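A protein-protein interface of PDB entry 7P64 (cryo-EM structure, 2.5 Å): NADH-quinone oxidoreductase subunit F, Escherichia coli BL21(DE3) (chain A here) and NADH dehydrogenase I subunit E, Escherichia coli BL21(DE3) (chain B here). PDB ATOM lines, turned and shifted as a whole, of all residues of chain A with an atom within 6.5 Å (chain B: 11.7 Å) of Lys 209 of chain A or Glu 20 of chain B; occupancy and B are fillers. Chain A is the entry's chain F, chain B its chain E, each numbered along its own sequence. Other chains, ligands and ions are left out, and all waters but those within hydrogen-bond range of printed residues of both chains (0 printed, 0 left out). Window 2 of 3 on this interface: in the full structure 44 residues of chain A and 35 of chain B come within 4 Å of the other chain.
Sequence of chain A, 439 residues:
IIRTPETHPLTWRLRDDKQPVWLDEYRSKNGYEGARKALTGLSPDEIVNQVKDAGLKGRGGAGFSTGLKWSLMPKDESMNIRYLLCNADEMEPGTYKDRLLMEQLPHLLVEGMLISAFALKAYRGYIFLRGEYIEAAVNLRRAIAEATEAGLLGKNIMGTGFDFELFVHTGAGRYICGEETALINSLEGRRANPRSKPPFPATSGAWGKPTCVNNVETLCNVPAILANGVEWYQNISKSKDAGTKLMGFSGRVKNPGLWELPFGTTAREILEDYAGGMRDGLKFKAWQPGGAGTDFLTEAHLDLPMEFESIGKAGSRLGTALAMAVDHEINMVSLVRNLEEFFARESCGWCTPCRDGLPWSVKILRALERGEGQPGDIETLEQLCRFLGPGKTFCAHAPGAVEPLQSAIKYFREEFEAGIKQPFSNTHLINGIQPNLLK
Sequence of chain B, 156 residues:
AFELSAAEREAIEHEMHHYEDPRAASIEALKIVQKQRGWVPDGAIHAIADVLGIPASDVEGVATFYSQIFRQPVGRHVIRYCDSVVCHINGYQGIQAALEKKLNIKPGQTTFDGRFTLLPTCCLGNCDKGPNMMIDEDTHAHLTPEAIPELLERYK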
ATOM      1  N   ILE A  81      -0.953  -8.363   6.015  1.00  0.00           N
ATOM      2  CA  ILE A  81      -0.498  -8.772   7.340  1.00  0.00           C
ATOM      3  C   ILE A  81       0.403  -7.689   7.919  1.00  0.00           C
ATOM      4  O   ILE A  81       1.432  -7.338   7.332  1.00  0.00           O
ATOM      5  CB  ILE A  81       0.229 -10.120   7.272  1.00  0.00           C
ATOM      6  CG1 ILE A  81      -0.744 -11.232   6.876  1.00  0.00           C
ATOM      7  CG2 ILE A  81       0.897 -10.435   8.593  1.00  0.00           C
ATOM      8  CD1 ILE A  81      -1.862 -11.442   7.869  1.00  0.00           C
ATOM      9  N   ARG A  82       0.020  -7.155   9.080  1.00  0.00           N
ATOM     10  CA  ARG A  82       0.772  -6.086   9.717  1.00  0.00           C
ATOM     11  C   ARG A  82       0.776  -6.270  11.228  1.00  0.00           C
ATOM     12  O   ARG A  82      -0.197  -6.759  11.827  1.00  0.00           O
ATOM     13  CB  ARG A  82       0.210  -4.711   9.348  1.00  0.00           C
ATOM     14  CG  ARG A  82       0.740  -4.168   8.039  1.00  0.00           C
ATOM     15  CD  ARG A  82      -0.183  -3.132   7.435  1.00  0.00           C
ATOM     16  NE  ARG A  82       0.132  -2.894   6.032  1.00  0.00           N
ATOM     17  CZ  ARG A  82       0.450  -1.712   5.525  1.00  0.00           C
ATOM     18  NH1 ARG A  82       0.500  -0.627   6.279  1.00  0.00           N
ATOM     19  NH2 ARG A  82       0.726  -1.616   4.227  1.00  0.00           N
ATOM     20  N   TYR A  83       1.885  -5.857  11.841  1.00  0.00           N
ATOM     21  CA  TYR A  83       2.115  -6.072  13.262  1.00  0.00           C
ATOM     22  C   TYR A  83       2.403  -4.760  13.975  1.00  0.00           C
ATOM     23  O   TYR A  83       3.164  -3.920  13.482  1.00  0.00           O
ATOM     24  CB  TYR A  83       3.267  -7.049  13.484  1.00  0.00           C
ATOM     25  CG  TYR A  83       2.957  -8.453  13.032  1.00  0.00           C
ATOM     26  CD1 TYR A  83       2.116  -9.267  13.774  1.00  0.00           C
ATOM     27  CD2 TYR A  83       3.497  -8.961  11.860  1.00  0.00           C
ATOM     28  CE1 TYR A  83       1.826 -10.550  13.366  1.00  0.00           C
ATOM     29  CE2 TYR A  83       3.212 -10.242  11.445  1.00  0.00           C
ATOM     30  CZ  TYR A  83       2.376 -11.031  12.201  1.00  0.00           C
ATOM     31  OH  TYR A  83       2.086 -12.310  11.791  1.00  0.00           O
ATOM     32  N   TYR A 123      -2.976  -6.062  11.701  1.00  0.00           N
ATOM     33  CA  TYR A 123      -3.868  -7.177  11.986  1.00  0.00           C
ATOM     34  C   TYR A 123      -3.558  -7.815  13.331  1.00  0.00           C
ATOM     35  O   TYR A 123      -4.454  -8.394  13.953  1.00  0.00           O
ATOM     36  CB  TYR A 123      -3.801  -8.201  10.851  1.00  0.00           C
ATOM     37  CG  TYR A 123      -3.143  -9.521  11.191  1.00  0.00           C
ATOM     38  CD1 TYR A 123      -1.760  -9.656  11.180  1.00  0.00           C
ATOM     39  CD2 TYR A 123      -3.909 -10.639  11.491  1.00  0.00           C
ATOM     40  CE1 TYR A 123      -1.162 -10.860  11.481  1.00  0.00           C
ATOM     41  CE2 TYR A 123      -3.317 -11.847  11.790  1.00  0.00           C
ATOM     42  CZ  TYR A 123      -1.944 -11.952  11.781  1.00  0.00           C
ATOM     43  OH  TYR A 123      -1.348 -13.154  12.079  1.00  0.00           O
ATOM     44  N   ARG A 124      -2.315  -7.722  13.807  1.00  0.00           N
ATOM     45  CA  ARG A 124      -1.998  -8.286  15.112  1.00  0.00           C
ATOM     46  C   ARG A 124      -1.166  -7.318  15.937  1.00  0.00           C
ATOM     47  O   ARG A 124      -0.429  -6.485  15.401  1.00  0.00           O
ATOM     48  CB  ARG A 124      -1.265  -9.623  14.990  1.00  0.00           C
ATOM     49  CG  ARG A 124      -2.126 -10.822  15.341  1.00  0.00           C
ATOM     50  CD  ARG A 124      -1.347 -12.114  15.234  1.00  0.00           C
ATOM     51  NE  ARG A 124      -2.171 -13.271  15.554  1.00  0.00           N
ATOM     52  CZ  ARG A 124      -1.837 -14.525  15.283  1.00  0.00           C
ATOM     53  NH1 ARG A 124      -0.701 -14.822  14.675  1.00  0.00           N
ATOM     54  NH2 ARG A 124      -2.664 -15.506  15.629  1.00  0.00           N
ATOM     55  N   TYR A 126       1.297  -7.112  19.672  1.00  0.00           N
ATOM     56  CA  TYR A 126       1.981  -7.770  20.774  1.00  0.00           C
ATOM     57  C   TYR A 126       2.487  -6.722  21.750  1.00  0.00           C
ATOM     58  O   TYR A 126       2.856  -5.616  21.356  1.00  0.00           O
ATOM     59  CB  TYR A 126       3.155  -8.626  20.285  1.00  0.00           C
ATOM     60  CG  TYR A 126       2.754  -9.783  19.407  1.00  0.00           C
ATOM     61  CD1 TYR A 126       2.405 -11.007  19.958  1.00  0.00           C
ATOM     62  CD2 TYR A 126       2.725  -9.653  18.028  1.00  0.00           C
ATOM     63  CE1 TYR A 126       2.038 -12.068  19.159  1.00  0.00           C
ATOM     64  CE2 TYR A 126       2.359 -10.708  17.222  1.00  0.00           C
ATOM     65  CZ  TYR A 126       2.016 -11.913  17.792  1.00  0.00           C
ATOM     66  OH  TYR A 126       1.652 -12.967  16.991  1.00  0.00           O
ATOM     67  N   PRO A 201      11.997  -1.364  10.227  1.00  0.00           N
ATOM     68  CA  PRO A 201      10.888  -2.288  10.525  1.00  0.00           C
ATOM     69  C   PRO A 201       9.556  -1.907   9.905  1.00  0.00           C
ATOM     70  O   PRO A 201       8.695  -2.783   9.761  1.00  0.00           O
ATOM     71  CB  PRO A 201      10.814  -2.255  12.055  1.00  0.00           C
ATOM     72  CG  PRO A 201      12.193  -1.964  12.473  1.00  0.00           C
ATOM     73  CD  PRO A 201      12.736  -1.007  11.453  1.00  0.00           C
ATOM     74  N   ALA A 202       9.354  -0.639   9.538  1.00  0.00           N
ATOM     75  CA  ALA A 202       8.117  -0.247   8.871  1.00  0.00           C
ATOM     76  C   ALA A 202       7.979  -0.903   7.503  1.00  0.00           C
ATOM     77  O   ALA A 202       6.859  -1.161   7.053  1.00  0.00           O
ATOM     78  CB  ALA A 202       8.052   1.273   8.740  1.00  0.00           C
ATOM     79  N   THR A 203       9.097  -1.187   6.837  1.00  0.00           N
ATOM     80  CA  THR A 203       9.082  -1.858   5.545  1.00  0.00           C
ATOM     81  C   THR A 203       9.077  -3.376   5.703  1.00  0.00           C
ATOM     82  O   THR A 203       8.235  -4.061   5.114  1.00  0.00           O
ATOM     83  CB  THR A 203      10.282  -1.390   4.709  1.00  0.00           C
ATOM     84  OG1 THR A 203       9.968  -0.136   4.094  1.00  0.00           O
ATOM     85  CG2 THR A 203      10.625  -2.394   3.615  1.00  0.00           C
ATOM     86  N   SER A 204       9.995  -3.917   6.507  1.00  0.00           N
ATOM     87  CA  SER A 204      10.051  -5.358   6.748  1.00  0.00           C
ATOM     88  C   SER A 204      10.514  -5.562   8.188  1.00  0.00           C
ATOM     89  O   SER A 204      11.715  -5.532   8.467  1.00  0.00           O
ATOM     90  CB  SER A 204      10.977  -6.050   5.757  1.00  0.00           C
ATOM     91  OG  SER A 204      12.326  -5.682   5.973  1.00  0.00           O
ATOM     92  N   GLY A 205       9.559  -5.768   9.089  1.00  0.00           N
ATOM     93  CA  GLY A 205       9.873  -5.930  10.492  1.00  0.00           C
ATOM     94  C   GLY A 205       9.693  -7.345  10.995  1.00  0.00           C
ATOM     95  O   GLY A 205      10.505  -8.223  10.695  1.00  0.00           O
ATOM     96  N   ALA A 206       8.628  -7.580  11.757  1.00  0.00           N
ATOM     97  CA  ALA A 206       8.401  -8.883  12.368  1.00  0.00           C
ATOM     98  C   ALA A 206       7.964  -9.886  11.312  1.00  0.00           C
ATOM     99  O   ALA A 206       6.952  -9.677  10.634  1.00  0.00           O
ATOM    100  CB  ALA A 206       7.359  -8.775  13.476  1.00  0.00           C
ATOM    101  N   TRP A 207       8.739 -10.966  11.178  1.00  0.00           N
ATOM    102  CA  TRP A 207       8.512 -12.037  10.204  1.00  0.00           C
ATOM    103  C   TRP A 207       8.462 -11.507   8.774  1.00  0.00           C
ATOM    104  O   TRP A 207       7.725 -12.026   7.934  1.00  0.00           O
ATOM    105  CB  TRP A 207       7.244 -12.832  10.532  1.00  0.00           C
ATOM    106  CG  TRP A 207       7.287 -13.489  11.872  1.00  0.00           C
ATOM    107  CD1 TRP A 207       7.983 -14.610  12.212  1.00  0.00           C
ATOM    108  CD2 TRP A 207       6.603 -13.069  13.056  1.00  0.00           C
ATOM    109  NE1 TRP A 207       7.776 -14.913  13.533  1.00  0.00           N
ATOM    110  CE2 TRP A 207       6.932 -13.982  14.075  1.00  0.00           C
ATOM    111  CE3 TRP A 207       5.744 -12.009  13.354  1.00  0.00           C
ATOM    112  CZ2 TRP A 207       6.433 -13.866  15.367  1.00  0.00           C
ATOM    113  CZ3 TRP A 207       5.251 -11.896  14.638  1.00  0.00           C
ATOM    114  CH2 TRP A 207       5.596 -12.820  15.628  1.00  0.00           C
ATOM    115  N   GLY A 208       9.239 -10.463   8.492  1.00  0.00           N
ATOM    116  CA  GLY A 208       9.282  -9.856   7.183  1.00  0.00           C
ATOM    117  C   GLY A 208       8.115  -8.955   6.852  1.00  0.00           C
ATOM    118  O   GLY A 208       8.131  -8.315   5.794  1.00  0.00           O
ATOM    119  N   LYS A 209       7.112  -8.879   7.712  1.00  0.00           N
ATOM    120  CA  LYS A 209       5.919  -8.084   7.496  1.00  0.00           C
ATOM    121  C   LYS A 209       6.139  -6.657   7.969  1.00  0.00           C
ATOM    122  O   LYS A 209       7.056  -6.387   8.748  1.00  0.00           O
ATOM    123  CB  LYS A 209       4.737  -8.703   8.236  1.00  0.00           C
ATOM    124  CG  LYS A 209       4.599 -10.193   8.031  1.00  0.00           C
ATOM    125  CD  LYS A 209       4.309 -10.526   6.583  1.00  0.00           C
ATOM    126  CE  LYS A 209       4.023 -12.005   6.417  1.00  0.00           C
ATOM    127  NZ  LYS A 209       5.208 -12.836   6.767  1.00  0.00           N
ATOM    128  N   PRO A 210       5.342  -5.711   7.474  1.00  0.00           N
ATOM    129  CA  PRO A 210       5.370  -4.357   8.038  1.00  0.00           C
ATOM    130  C   PRO A 210       4.999  -4.349   9.516  1.00  0.00           C
ATOM    131  O   PRO A 210       3.969  -4.895   9.931  1.00  0.00           O
ATOM    132  CB  PRO A 210       4.350  -3.592   7.184  1.00  0.00           C
ATOM    133  CG  PRO A 210       3.830  -4.564   6.170  1.00  0.00           C
ATOM    134  CD  PRO A 210       4.734  -5.732   6.137  1.00  0.00           C
ATOM    135  N   THR A 211       5.861  -3.718  10.309  1.00  0.00           N
ATOM    136  CA  THR A 211       5.795  -3.752  11.760  1.00  0.00           C
ATOM    137  C   THR A 211       6.097  -2.364  12.298  1.00  0.00           C
ATOM    138  O   THR A 211       7.007  -1.688  11.811  1.00  0.00           O
ATOM    139  CB  THR A 211       6.799  -4.764  12.330  1.00  0.00           C
ATOM    140  OG1 THR A 211       6.633  -6.024  11.673  1.00  0.00           O
ATOM    141  CG2 THR A 211       6.592  -4.956  13.811  1.00  0.00           C
ATOM    142  N   ILE B  12       3.043 -25.519  25.608  1.00  0.00           N
ATOM    143  CA  ILE B  12       3.943 -25.132  24.525  1.00  0.00           C
ATOM    144  C   ILE B  12       3.187 -25.038  23.205  1.00  0.00           C
ATOM    145  O   ILE B  12       3.355 -24.073  22.453  1.00  0.00           O
ATOM    146  CB  ILE B  12       5.130 -26.110  24.444  1.00  0.00           C
ATOM    147  CG1 ILE B  12       6.089 -25.876  25.610  1.00  0.00           C
ATOM    148  CG2 ILE B  12       5.882 -25.946  23.144  1.00  0.00           C
ATOM    149  CD1 ILE B  12       7.142 -26.943  25.752  1.00  0.00           C
ATOM    150  N   GLU B  13       2.318 -26.015  22.919  1.00  0.00           N
ATOM    151  CA  GLU B  13       1.544 -25.987  21.679  1.00  0.00           C
ATOM    152  C   GLU B  13       0.573 -24.811  21.646  1.00  0.00           C
ATOM    153  O   GLU B  13       0.392 -24.172  20.599  1.00  0.00           O
ATOM    154  CB  GLU B  13       0.800 -27.309  21.502  1.00  0.00           C
ATOM    155  CG  GLU B  13       1.671 -28.430  20.962  1.00  0.00           C
ATOM    156  CD  GLU B  13       1.241 -29.798  21.451  1.00  0.00           C
ATOM    157  OE1 GLU B  13       0.300 -29.873  22.270  1.00  0.00           O
ATOM    158  OE2 GLU B  13       1.841 -30.801  21.015  1.00  0.00           O
ATOM    159  N   HIS B  14      -0.048 -24.498  22.787  1.00  0.00           N
ATOM    160  CA  HIS B  14      -0.904 -23.320  22.859  1.00  0.00           C
ATOM    161  C   HIS B  14      -0.106 -22.037  22.668  1.00  0.00           C
ATOM    162  O   HIS B  14      -0.635 -21.052  22.140  1.00  0.00           O
ATOM    163  CB  HIS B  14      -1.650 -23.292  24.192  1.00  0.00           C
ATOM    164  CG  HIS B  14      -2.630 -22.168  24.310  1.00  0.00           C
ATOM    165  ND1 HIS B  14      -3.742 -22.063  23.502  1.00  0.00           N
ATOM    166  CD2 HIS B  14      -2.664 -21.097  25.137  1.00  0.00           C
ATOM    167  CE1 HIS B  14      -4.419 -20.978  23.828  1.00  0.00           C
ATOM    168  NE2 HIS B  14      -3.788 -20.373  24.817  1.00  0.00           N
ATOM    169  N   GLU B  15       1.162 -22.024  23.088  1.00  0.00           N
ATOM    170  CA  GLU B  15       2.011 -20.872  22.809  1.00  0.00           C
ATOM    171  C   GLU B  15       2.351 -20.773  21.325  1.00  0.00           C
ATOM    172  O   GLU B  15       2.404 -19.669  20.771  1.00  0.00           O
ATOM    173  CB  GLU B  15       3.282 -20.933  23.653  1.00  0.00           C
ATOM    174  CG  GLU B  15       3.084 -20.456  25.079  1.00  0.00           C
ATOM    175  CD  GLU B  15       2.438 -19.085  25.148  1.00  0.00           C
ATOM    176  OE1 GLU B  15       2.990 -18.134  24.558  1.00  0.00           O
ATOM    177  OE2 GLU B  15       1.374 -18.959  25.790  1.00  0.00           O
ATOM    178  N   MET B  16       2.589 -21.911  20.664  1.00  0.00           N
ATOM    179  CA  MET B  16       2.794 -21.888  19.213  1.00  0.00           C
ATOM    180  C   MET B  16       1.543 -21.478  18.451  1.00  0.00           C
ATOM    181  O   MET B  16       1.656 -21.036  17.304  1.00  0.00           O
ATOM    182  CB  MET B  16       3.280 -23.240  18.674  1.00  0.00           C
ATOM    183  CG  MET B  16       4.332 -23.941  19.496  1.00  0.00           C
ATOM    184  SD  MET B  16       4.492 -25.697  19.118  1.00  0.00           S
ATOM    185  CE  MET B  16       4.283 -25.690  17.342  1.00  0.00           C
ATOM    186  N   HIS B  17       0.358 -21.617  19.050  1.00  0.00           N
ATOM    187  CA  HIS B  17      -0.847 -21.096  18.410  1.00  0.00           C
ATOM    188  C   HIS B  17      -0.866 -19.572  18.325  1.00  0.00           C
ATOM    189  O   HIS B  17      -1.620 -19.021  17.516  1.00  0.00           O
ATOM    190  CB  HIS B  17      -2.096 -21.576  19.151  1.00  0.00           C
ATOM    191  CG  HIS B  17      -2.360 -23.041  19.002  1.00  0.00           C
ATOM    192  ND1 HIS B  17      -3.153 -23.747  19.880  1.00  0.00           N
ATOM    193  CD2 HIS B  17      -1.938 -23.933  18.076  1.00  0.00           C
ATOM    194  CE1 HIS B  17      -3.206 -25.012  19.502  1.00  0.00           C
ATOM    195  NE2 HIS B  17      -2.477 -25.151  18.410  1.00  0.00           N
ATOM    196  N   HIS B  18      -0.059 -18.878  19.130  1.00  0.00           N
ATOM    197  CA  HIS B  18      -0.107 -17.423  19.206  1.00  0.00           C
ATOM    198  C   HIS B  18       0.687 -16.727  18.109  1.00  0.00           C
ATOM    199  O   HIS B  18       0.529 -15.515  17.934  1.00  0.00           O
ATOM    200  CB  HIS B  18       0.416 -16.946  20.565  1.00  0.00           C
ATOM    201  CG  HIS B  18      -0.447 -17.337  21.723  1.00  0.00           C
ATOM    202  ND1 HIS B  18      -1.602 -18.075  21.580  1.00  0.00           N
ATOM    203  CD2 HIS B  18      -0.318 -17.096  23.048  1.00  0.00           C
ATOM    204  CE1 HIS B  18      -2.148 -18.270  22.767  1.00  0.00           C
ATOM    205  NE2 HIS B  18      -1.388 -17.686  23.675  1.00  0.00           N
ATOM    206  N   TYR B  19       1.533 -17.444  17.377  1.00  0.00           N
ATOM    207  CA  TYR B  19       2.435 -16.831  16.415  1.00  0.00           C
ATOM    208  C   TYR B  19       2.290 -17.501  15.057  1.00  0.00           C
ATOM    209  O   TYR B  19       1.826 -18.638  14.947  1.00  0.00           O
ATOM    210  CB  TYR B  19       3.896 -16.923  16.872  1.00  0.00           C
ATOM    211  CG  TYR B  19       4.134 -16.472  18.292  1.00  0.00           C
ATOM    212  CD1 TYR B  19       4.305 -15.129  18.591  1.00  0.00           C
ATOM    213  CD2 TYR B  19       4.199 -17.389  19.331  1.00  0.00           C
ATOM    214  CE1 TYR B  19       4.527 -14.711  19.883  1.00  0.00           C
ATOM    215  CE2 TYR B  19       4.420 -16.979  20.628  1.00  0.00           C
ATOM    216  CZ  TYR B  19       4.584 -15.638  20.898  1.00  0.00           C
ATOM    217  OH  TYR B  19       4.804 -15.220  22.188  1.00  0.00           O
ATOM    218  N   GLU B  20       2.706 -16.778  14.019  1.00  0.00           N
ATOM    219  CA  GLU B  20       2.720 -17.320  12.668  1.00  0.00           C
ATOM    220  C   GLU B  20       3.942 -18.187  12.393  1.00  0.00           C
ATOM    221  O   GLU B  20       4.027 -18.786  11.316  1.00  0.00           O
ATOM    222  CB  GLU B  20       2.656 -16.185  11.646  1.00  0.00           C
ATOM    223  CG  GLU B  20       3.787 -15.186  11.759  1.00  0.00           C
ATOM    224  CD  GLU B  20       4.142 -14.567  10.427  1.00  0.00           C
ATOM    225  OE1 GLU B  20       4.994 -15.137   9.715  1.00  0.00           O
ATOM    226  OE2 GLU B  20       3.569 -13.512  10.089  1.00  0.00           O
ATOM    227  N   ASP B  21       4.884 -18.259  13.332  1.00  0.00           N
ATOM    228  CA  ASP B  21       6.060 -19.105  13.225  1.00  0.00           C
ATOM    229  C   ASP B  21       6.213 -19.863  14.538  1.00  0.00           C
ATOM    230  O   ASP B  21       6.208 -19.238  15.612  1.00  0.00           O
ATOM    231  CB  ASP B  21       7.311 -18.270  12.929  1.00  0.00           C
ATOM    232  CG  ASP B  21       8.389 -19.056  12.210  1.00  0.00           C
ATOM    233  OD1 ASP B  21       9.024 -18.488  11.299  1.00  0.00           O
ATOM    234  OD2 ASP B  21       8.618 -20.230  12.560  1.00  0.00           O
ATOM    235  N   PRO B  22       6.323 -21.194  14.506  1.00  0.00           N
ATOM    236  CA  PRO B  22       6.503 -21.949  15.759  1.00  0.00           C
ATOM    237  C   PRO B  22       7.811 -21.666  16.478  1.00  0.00           C
ATOM    238  O   PRO B  22       7.914 -21.974  17.670  1.00  0.00           O
ATOM    239  CB  PRO B  22       6.425 -23.413  15.303  1.00  0.00           C
ATOM    240  CG  PRO B  22       6.642 -23.378  13.829  1.00  0.00           C
ATOM    241  CD  PRO B  22       6.067 -22.085  13.364  1.00  0.00           C
ATOM    242  N   ARG B  23       8.811 -21.100  15.797  1.00  0.00           N
ATOM    243  CA  ARG B  23      10.065 -20.748  16.456  1.00  0.00           C
ATOM    244  C   ARG B  23       9.865 -19.652  17.495  1.00  0.00           C
ATOM    245  O   ARG B  23      10.608 -19.586  18.481  1.00  0.00           O
ATOM    246  CB  ARG B  23      11.095 -20.311  15.413  1.00  0.00           C
ATOM    247  CG  ARG B  23      12.493 -20.089  15.959  1.00  0.00           C
ATOM    248  CD  ARG B  23      13.281 -19.141  15.085  1.00  0.00           C
ATOM    249  NE  ARG B  23      13.552 -19.724  13.780  1.00  0.00           N
ATOM    250  CZ  ARG B  23      14.557 -20.548  13.521  1.00  0.00           C
ATOM    251  NH1 ARG B  23      15.419 -20.900  14.460  1.00  0.00           N
ATOM    252  NH2 ARG B  23      14.702 -21.029  12.291  1.00  0.00           N
ATOM    253  N   ALA B  24       8.846 -18.811  17.316  1.00  0.00           N
ATOM    254  CA  ALA B  24       8.593 -17.686  18.207  1.00  0.00           C
ATOM    255  C   ALA B  24       8.130 -18.105  19.596  1.00  0.00           C
ATOM    256  O   ALA B  24       8.063 -17.253  20.486  1.00  0.00           O
ATOM    257  CB  ALA B  24       7.562 -16.752  17.577  1.00  0.00           C
ATOM    258  N   ALA B  25       7.807 -19.377  19.805  1.00  0.00           N
ATOM    259  CA  ALA B  25       7.420 -19.883  21.113  1.00  0.00           C
ATOM    260  C   ALA B  25       8.579 -20.527  21.865  1.00  0.00           C
ATOM    261  O   ALA B  25       8.343 -21.231  22.849  1.00  0.00           O
ATOM    262  CB  ALA B  25       6.272 -20.881  20.972  1.00  0.00           C
ATOM    263  N   SER B  26       9.821 -20.303  21.428  1.00  0.00           N
ATOM    264  CA  SER B  26      10.964 -20.956  22.062  1.00  0.00           C
ATOM    265  C   SER B  26      11.241 -20.393  23.449  1.00  0.00           C
ATOM    266  O   SER B  26      11.510 -21.152  24.388  1.00  0.00           O
ATOM    267  CB  SER B  26      12.200 -20.826  21.175  1.00  0.00           C
ATOM    268  OG  SER B  26      12.547 -19.468  20.982  1.00  0.00           O
ATOM    269  N   LEU B  52       9.002 -27.969  18.702  1.00  0.00           N
ATOM    270  CA  LEU B  52       8.888 -26.749  17.914  1.00  0.00           C
ATOM    271  C   LEU B  52       9.279 -26.924  16.454  1.00  0.00           C
ATOM    272  O   LEU B  52       8.903 -26.089  15.626  1.00  0.00           O
ATOM    273  CB  LEU B  52       9.754 -25.654  18.528  1.00  0.00           C
ATOM    274  CG  LEU B  52       9.056 -24.627  19.408  1.00  0.00           C
ATOM    275  CD1 LEU B  52       8.590 -25.247  20.704  1.00  0.00           C
ATOM    276  CD2 LEU B  52      10.028 -23.524  19.679  1.00  0.00           C
ATOM    277  N   GLY B  53      10.025 -27.970  16.116  1.00  0.00           N
ATOM    278  CA  GLY B  53      10.493 -28.124  14.754  1.00  0.00           C
ATOM    279  C   GLY B  53      11.651 -27.227  14.380  1.00  0.00           C
ATOM    280  O   GLY B  53      11.769 -26.833  13.216  1.00  0.00           O
ATOM    281  N   ILE B  54      12.503 -26.887  15.335  1.00  0.00           N
ATOM    282  CA  ILE B  54      13.690 -26.076  15.082  1.00  0.00           C
ATOM    283  C   ILE B  54      14.892 -26.874  15.565  1.00  0.00           C
ATOM    284  O   ILE B  54      14.737 -27.838  16.334  1.00  0.00           O
ATOM    285  CB  ILE B  54      13.594 -24.688  15.758  1.00  0.00           C
ATOM    286  CG1 ILE B  54      13.375 -24.821  17.262  1.00  0.00           C
ATOM    287  CG2 ILE B  54      12.496 -23.852  15.116  1.00  0.00           C
ATOM    288  CD1 ILE B  54      13.353 -23.493  17.970  1.00  0.00           C
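Arg 124 of chain A touches His 18 of chain B (NH1 to O, 3.6 Å). Glu 20 of chain B touches Arg 124 of chain A (N to NH1, 3.98 Å). Tyr 19 of chain B touches Tyr 126 of chain A. Trp 207 of chain A touches Tyr 19 of chain B. OE1 of Glu 20 of chain B touches CB of Trp 207 of chain A, 3.3 Å away. Trp 207 of chain A touches Asp 21 of chain B (NE1 to CB, 3.4 Å). Trp 207 of chain A touches Ala 24 of chain B.
The side-chain carboxylate of Glu 20 of chain B sits at hydrogen-bond distance from the side-chain hydroxyl of Tyr 83 of chain A (2.6 Å). The side-chain amino group (NZ) of Lys 209 of chain A is in salt-bridge range of the side-chain carboxylate (OE1) of Glu 20 of chain B (3.7 Å). The backbone carbonyl oxygen (O) of His 18 of chain B sits at hydrogen-bond distance from the side-chain hydroxyl (OH) of Tyr 126 of chain A.
The backbone carbonyl oxygen of His 14 of chain B lies within hydrogen-bond range of a ring nitrogen (ND1) of His 18 of chain B (3.2 Å). NZ of Lys 209 of chain A sits at hydrogen-bond distance from O of Trp 207 of chain A (2.9 Å). O of Pro 210 of chain A is in hydrogen-bond range of N of Tyr 83 of chain A (3.0 Å). The side-chain hydroxyl (OH) of Tyr 123 of chain A lies within hydrogen-bond range of the guanidinium group (NH1) of Arg 124 of chain A. The backbone carbonyl oxygen (O) of Lys 209 of chain A lies within hydrogen-bond range of the side-chain hydroxyl (OG1) of Thr 211 of chain A (3.0 Å). O of Arg 82 of chain A is in hydrogen-bond range of N of Arg 124 of chain A, 3.1 Å away.
Of the 18 printed residues of chain B, 5 touch a printed residue of chain A. Printed residues of chain B that touch a printed residue of chain A: His 18, Tyr 19, Glu 20, Asp 21 and Ala 24. Hydrophobic or aromatic side chains of chain B that line the printed part of chain A: Tyr 19 and Ala 24. Along chain B the printed residues that touch a printed residue of chain A span positions 18 to 24. Of the 17 printed residues of chain A, 5 touch a printed residue of chain B. Among the printed residues, 10 pairs touch across the chains.
Lys 209 of chain A touches one residue of chain B. Of the printed residues of chain A, Glu 20 of chain B touches Tyr 83, Arg 124, Trp 207 and Lys 209. No residue of chain B comes within 4 Å of Ser 204 of chain A. No residue of chain B comes within 4 Å of Gly 205 of chain A. No residue of chain B comes within 4 Å of Ala 206 of chain A. Trp 207 of chain A touches four residues of chain B. No residue of chain B comes within 4 Å of Gly 208 of chain A. Pro 210 of chain A touches none of the printed residues of chain B. Of the printed residues of chain B, Arg 124 of chain A touches His 18 (3.6 Å) and Glu 20 (3.98 Å). Of the printed residues of chain A, Ala 24 of chain B touches Trp 207. Of the printed residues of chain B, Tyr 126 of chain A touches His 18 (2.9 Å) and Tyr 19 (3.7 Å). The nearest residue of chain B that does not touch Lys 209 of chain A is Asp 21 of chain B (8.2 Å). The nearest printed residue of chain A that does not touch Glu 20 of chain B is Ile 81 of chain A (4.3 Å).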
